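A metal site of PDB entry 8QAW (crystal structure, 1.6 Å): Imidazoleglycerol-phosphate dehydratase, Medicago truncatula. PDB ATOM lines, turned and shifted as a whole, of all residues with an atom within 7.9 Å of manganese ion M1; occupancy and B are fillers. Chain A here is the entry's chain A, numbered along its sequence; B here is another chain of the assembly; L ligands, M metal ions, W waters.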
ATOM      1  N   PHE A  43       5.456   2.209 -14.671  1.00  0.00           N
ATOM      2  CA  PHE A  43       6.465   1.163 -14.551  1.00  0.00           C
ATOM      3  C   PHE A  43       5.902  -0.055 -13.820  1.00  0.00           C
ATOM      4  O   PHE A  43       6.224  -1.196 -14.170  1.00  0.00           O
ATOM      5  CB  PHE A  43       7.722   1.676 -13.868  1.00  0.00           C
ATOM      6  CG  PHE A  43       8.843   0.669 -13.870  1.00  0.00           C
ATOM      7  CD1 PHE A  43       9.622   0.490 -14.996  1.00  0.00           C
ATOM      8  CD2 PHE A  43       9.072  -0.118 -12.768  1.00  0.00           C
ATOM      9  CE1 PHE A  43      10.639  -0.445 -15.005  1.00  0.00           C
ATOM     10  CE2 PHE A  43      10.095  -1.048 -12.772  1.00  0.00           C
ATOM     11  CZ  PHE A  43      10.868  -1.219 -13.898  1.00  0.00           C
ATOM     12  N   HIS A  46       4.088  -2.139 -16.283  1.00  0.00           N
ATOM     13  CA  HIS A  46       5.044  -2.935 -17.049  1.00  0.00           C
ATOM     14  C   HIS A  46       5.464  -4.184 -16.260  1.00  0.00           C
ATOM     15  O   HIS A  46       5.612  -5.264 -16.835  1.00  0.00           O
ATOM     16  CB  HIS A  46       6.246  -2.046 -17.403  1.00  0.00           C
ATOM     17  CG  HIS A  46       7.305  -2.712 -18.227  1.00  0.00           C
ATOM     18  ND1 HIS A  46       7.023  -3.552 -19.281  1.00  0.00           N
ATOM     19  CD2 HIS A  46       8.656  -2.613 -18.180  1.00  0.00           C
ATOM     20  CE1 HIS A  46       8.149  -3.974 -19.828  1.00  0.00           C
ATOM     21  NE2 HIS A  46       9.166  -3.417 -19.176  1.00  0.00           N
ATOM     22  N   MET A  47       5.651  -4.040 -14.945  1.00  0.00           N
ATOM     23  CA  MET A  47       6.012  -5.185 -14.121  1.00  0.00           C
ATOM     24  C   MET A  47       4.841  -6.158 -13.967  1.00  0.00           C
ATOM     25  O   MET A  47       5.024  -7.375 -14.038  1.00  0.00           O
ATOM     26  CB  MET A  47       6.505  -4.707 -12.760  1.00  0.00           C
ATOM     27  CG  MET A  47       7.805  -3.902 -12.838  1.00  0.00           C
ATOM     28  SD  MET A  47       9.167  -4.778 -13.628  1.00  0.00           S
ATOM     29  CE  MET A  47       9.108  -4.110 -15.296  1.00  0.00           C
ATOM     30  N   GLN A  50       4.441  -8.655 -16.643  1.00  0.00           N
ATOM     31  CA  GLN A  50       5.258  -9.857 -16.593  1.00  0.00           C
ATOM     32  C   GLN A  50       4.530 -11.010 -15.922  1.00  0.00           C
ATOM     33  O   GLN A  50       4.783 -12.180 -16.244  1.00  0.00           O
ATOM     34  CB  GLN A  50       6.574  -9.590 -15.858  1.00  0.00           C
ATOM     35  CG  GLN A  50       7.277  -8.349 -16.302  1.00  0.00           C
ATOM     36  CD  GLN A  50       7.563  -8.304 -17.779  1.00  0.00           C
ATOM     37  OE1 GLN A  50       7.357  -7.273 -18.417  1.00  0.00           O
ATOM     38  NE2 GLN A  50       8.061  -9.393 -18.333  1.00  0.00           N
ATOM     39  N   LEU A 106      17.943 -11.389 -16.911  1.00  0.00           N
ATOM     40  CA  LEU A 106      17.608 -10.347 -17.887  1.00  0.00           C
ATOM     41  C   LEU A 106      18.927  -9.647 -18.166  1.00  0.00           C
ATOM     42  O   LEU A 106      19.376  -8.823 -17.355  1.00  0.00           O
ATOM     43  CB  LEU A 106      16.529  -9.385 -17.390  1.00  0.00           C
ATOM     44  CG  LEU A 106      15.797  -8.579 -18.486  1.00  0.00           C
ATOM     45  CD1 LEU A 106      14.758  -7.641 -17.877  1.00  0.00           C
ATOM     46  CD2 LEU A 106      16.729  -7.792 -19.429  1.00  0.00           C
ATOM     47  N   HIS A 168      16.239  -1.129 -14.028  1.00  0.00           N
ATOM     48  CA  HIS A 168      15.113  -1.665 -14.811  1.00  0.00           C
ATOM     49  C   HIS A 168      15.283  -3.179 -15.017  1.00  0.00           C
ATOM     50  O   HIS A 168      14.351  -3.947 -14.790  1.00  0.00           O
ATOM     51  CB  HIS A 168      15.016  -0.885 -16.134  1.00  0.00           C
ATOM     52  CG  HIS A 168      13.849  -1.210 -17.021  1.00  0.00           C
ATOM     53  ND1 HIS A 168      13.168  -0.239 -17.713  1.00  0.00           N
ATOM     54  CD2 HIS A 168      13.309  -2.392 -17.403  1.00  0.00           C
ATOM     55  CE1 HIS A 168      12.233  -0.806 -18.471  1.00  0.00           C
ATOM     56  NE2 HIS A 168      12.289  -2.114 -18.284  1.00  0.00           N
ATOM     57  N   HIS A 169      16.497  -3.614 -15.370  1.00  0.00           N
ATOM     58  CA  HIS A 169      16.737  -5.061 -15.543  1.00  0.00           C
ATOM     59  C   HIS A 169      16.526  -5.825 -14.245  1.00  0.00           C
ATOM     60  O   HIS A 169      15.909  -6.900 -14.244  1.00  0.00           O
ATOM     61  CB  HIS A 169      18.151  -5.302 -16.061  1.00  0.00           C
ATOM     62  CG  HIS A 169      18.352  -4.920 -17.489  1.00  0.00           C
ATOM     63  ND1 HIS A 169      19.582  -5.008 -18.112  1.00  0.00           N
ATOM     64  CD2 HIS A 169      17.482  -4.464 -18.426  1.00  0.00           C
ATOM     65  CE1 HIS A 169      19.449  -4.621 -19.373  1.00  0.00           C
ATOM     66  NE2 HIS A 169      18.192  -4.292 -19.582  1.00  0.00           N
ATOM     67  N   GLU A 172      12.748  -5.951 -13.392  1.00  0.00           N
ATOM     68  CA  GLU A 172      12.009  -6.766 -14.349  1.00  0.00           C
ATOM     69  C   GLU A 172      12.361  -8.238 -14.208  1.00  0.00           C
ATOM     70  O   GLU A 172      11.469  -9.093 -14.270  1.00  0.00           O
ATOM     71  CB  GLU A 172      12.268  -6.277 -15.771  1.00  0.00           C
ATOM     72  CG  GLU A 172      11.367  -6.962 -16.797  1.00  0.00           C
ATOM     73  CD  GLU A 172      11.442  -6.338 -18.181  1.00  0.00           C
ATOM     74  OE1 GLU A 172      11.674  -5.114 -18.261  1.00  0.00           O
ATOM     75  OE2 GLU A 172      11.249  -7.061 -19.178  1.00  0.00           O
ATOM     76  N   LYS A 176       9.792 -11.313 -13.498  1.00  0.00           N
ATOM     77  CA  LYS A 176       9.767 -12.531 -14.313  1.00  0.00           C
ATOM     78  C   LYS A 176       9.925 -13.768 -13.448  1.00  0.00           C
ATOM     79  O   LYS A 176       9.188 -14.754 -13.594  1.00  0.00           O
ATOM     80  CB  LYS A 176      10.851 -12.479 -15.385  1.00  0.00           C
ATOM     81  CG  LYS A 176      10.623 -11.416 -16.433  1.00  0.00           C
ATOM     82  CD  LYS A 176      11.658 -11.476 -17.521  1.00  0.00           C
ATOM     83  CE  LYS A 176      11.470 -10.322 -18.519  1.00  0.00           C
ATOM     84  NZ  LYS A 176      12.328 -10.489 -19.710  1.00  0.00           N
ATOM     85  N   GLU B  20       6.553  -1.943 -28.098  1.00  0.00           N
ATOM     86  CA  GLU B  20       7.109  -0.901 -27.243  1.00  0.00           C
ATOM     87  C   GLU B  20       7.609   0.321 -28.010  1.00  0.00           C
ATOM     88  O   GLU B  20       7.539   1.435 -27.481  1.00  0.00           O
ATOM     89  CB  GLU B  20       8.279  -1.440 -26.401  1.00  0.00           C
ATOM     90  CG  GLU B  20       7.903  -2.497 -25.394  1.00  0.00           C
ATOM     91  CD  GLU B  20       8.154  -3.903 -25.893  1.00  0.00           C
ATOM     92  OE1 GLU B  20       8.353  -4.082 -27.110  1.00  0.00           O
ATOM     93  OE2 GLU B  20       8.162  -4.838 -25.054  1.00  0.00           O
ATOM     94  N   ASP B  66       7.521   3.826 -25.667  1.00  0.00           N
ATOM     95  CA  ASP B  66       6.820   3.846 -24.381  1.00  0.00           C
ATOM     96  C   ASP B  66       7.580   4.649 -23.339  1.00  0.00           C
ATOM     97  O   ASP B  66       7.839   4.162 -22.231  1.00  0.00           O
ATOM     98  CB  ASP B  66       6.546   2.415 -23.899  1.00  0.00           C
ATOM     99  CG  ASP B  66       7.800   1.534 -23.856  1.00  0.00           C
ATOM    100  OD1 ASP B  66       8.934   2.028 -24.059  1.00  0.00           O
ATOM    101  OD2 ASP B  66       7.622   0.322 -23.599  1.00  0.00           O
ATOM    102  N   ILE B  69       6.819   4.870 -19.608  1.00  0.00           N
ATOM    103  CA  ILE B  69       7.385   3.967 -18.620  1.00  0.00           C
ATOM    104  C   ILE B  69       8.732   4.504 -18.153  1.00  0.00           C
ATOM    105  O   ILE B  69       8.922   4.855 -16.981  1.00  0.00           O
ATOM    106  CB  ILE B  69       7.516   2.548 -19.198  1.00  0.00           C
ATOM    107  CG1 ILE B  69       6.149   1.954 -19.556  1.00  0.00           C
ATOM    108  CG2 ILE B  69       8.296   1.632 -18.236  1.00  0.00           C
ATOM    109  CD1 ILE B  69       6.236   0.644 -20.287  1.00  0.00           C
ATOM    110  N   ASP B  70       9.675   4.557 -19.067  1.00  0.00           N
ATOM    111  CA  ASP B  70      10.966   5.224 -18.923  1.00  0.00           C
ATOM    112  C   ASP B  70      11.575   5.237 -20.318  1.00  0.00           C
ATOM    113  O   ASP B  70      10.920   4.852 -21.302  1.00  0.00           O
ATOM    114  CB  ASP B  70      11.840   4.565 -17.839  1.00  0.00           C
ATOM    115  CG  ASP B  70      12.376   3.185 -18.240  1.00  0.00           C
ATOM    116  OD1 ASP B  70      12.002   2.653 -19.304  1.00  0.00           O
ATOM    117  OD2 ASP B  70      13.191   2.628 -17.444  1.00  0.00           O
ATOM    118  N   HIS B  72      14.089   3.472 -21.319  1.00  0.00           N
ATOM    119  CA  HIS B  72      14.927   2.291 -21.505  1.00  0.00           C
ATOM    120  C   HIS B  72      14.643   1.595 -22.830  1.00  0.00           C
ATOM    121  O   HIS B  72      15.573   1.308 -23.608  1.00  0.00           O
ATOM    122  CB  HIS B  72      14.702   1.332 -20.329  1.00  0.00           C
ATOM    123  CG  HIS B  72      15.602   0.144 -20.330  1.00  0.00           C
ATOM    124  ND1 HIS B  72      16.464  -0.133 -19.287  1.00  0.00           N
ATOM    125  CD2 HIS B  72      15.755  -0.872 -21.225  1.00  0.00           C
ATOM    126  CE1 HIS B  72      17.110  -1.256 -19.547  1.00  0.00           C
ATOM    127  NE2 HIS B  72      16.703  -1.722 -20.717  1.00  0.00           N
ATOM    128  N   HIS B  73      13.372   1.275 -23.105  1.00  0.00           N
ATOM    129  CA  HIS B  73      13.082   0.496 -24.314  1.00  0.00           C
ATOM    130  C   HIS B  73      13.446   1.286 -25.571  1.00  0.00           C
ATOM    131  O   HIS B  73      14.017   0.729 -26.509  1.00  0.00           O
ATOM    132  CB  HIS B  73      11.617   0.058 -24.348  1.00  0.00           C
ATOM    133  CG  HIS B  73      11.195  -0.788 -23.194  1.00  0.00           C
ATOM    134  ND1 HIS B  73       9.888  -0.928 -22.812  1.00  0.00           N
ATOM    135  CD2 HIS B  73      11.912  -1.548 -22.329  1.00  0.00           C
ATOM    136  CE1 HIS B  73       9.802  -1.727 -21.759  1.00  0.00           C
ATOM    137  NE2 HIS B  73      11.022  -2.126 -21.443  1.00  0.00           N
ATOM    138  N   GLU B  76      17.242   1.401 -25.949  1.00  0.00           N
ATOM    139  CA  GLU B  76      17.758   0.108 -26.373  1.00  0.00           C
ATOM    140  C   GLU B  76      17.452  -0.148 -27.848  1.00  0.00           C
ATOM    141  O   GLU B  76      18.324  -0.568 -28.607  1.00  0.00           O
ATOM    142  CB  GLU B  76      17.161  -0.989 -25.499  1.00  0.00           C
ATOM    143  CG  GLU B  76      17.565  -2.381 -25.903  1.00  0.00           C
ATOM    144  CD  GLU B  76      17.354  -3.403 -24.801  1.00  0.00           C
ATOM    145  OE1 GLU B  76      16.864  -3.040 -23.690  1.00  0.00           O
ATOM    146  OE2 GLU B  76      17.687  -4.590 -25.036  1.00  0.00           O
HETATM  147  C1  LIG L   1      14.484  -3.950 -20.550  1.00  0.00           C
HETATM  148  O1  LIG L   1      15.372  -4.384 -21.296  1.00  0.00           O
HETATM  149  O2  LIG L   1      13.281  -4.120 -20.754  1.00  0.00           O
HETATM  150 MN    MN M   1      11.355  -3.593 -19.748  1.00  0.00          MN
HETATM  151 MN    MN M   2      17.407  -3.639 -21.604  1.00  0.00          MN
HETATM  152  O   HOH W   1      10.662  -5.367 -21.120  1.00  0.00           O
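ND1 of His 168 lies within hydrogen-bond range of OD2 of Asp 70 of chain B (2.9 Å). The side-chain amide oxygen (OE1) of Gln 50 sits close to the backbone carbonyl oxygen (O) of His 46, at 3.1 Å. The backbone NH (N) of Glu 172 lies close to the side-chain sulfur (SD) of Met 47, 3.8 Å away. A ring nitrogen (ND1) of His 73 of chain B sits at hydrogen-bond distance from the side-chain carboxylate of Asp 66 of chain B, at 2.7 Å. OE2 of Glu 172 lies within salt-bridge range of NZ of Lys 176, 3.6 Å away.
Within 4 Å of manganese ion M1: His 46, His 168, Glu 172 and His 73 of chain B. Along chain A the residues within 4 Å of manganese ion M1 span positions 46 to 172.
Manganese ion M1 is bound by OE1 of Glu 172 (2.2 Å), O2 of the ligand (2.2 Å), NE2 of His 73 of chain B (2.3 Å), NE2 of His 46 (2.3 Å), NE2 of His 168 (2.3 Å) and water W1 (2.3 Å). Manganese ion M1 has six donor atoms within binding distance.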
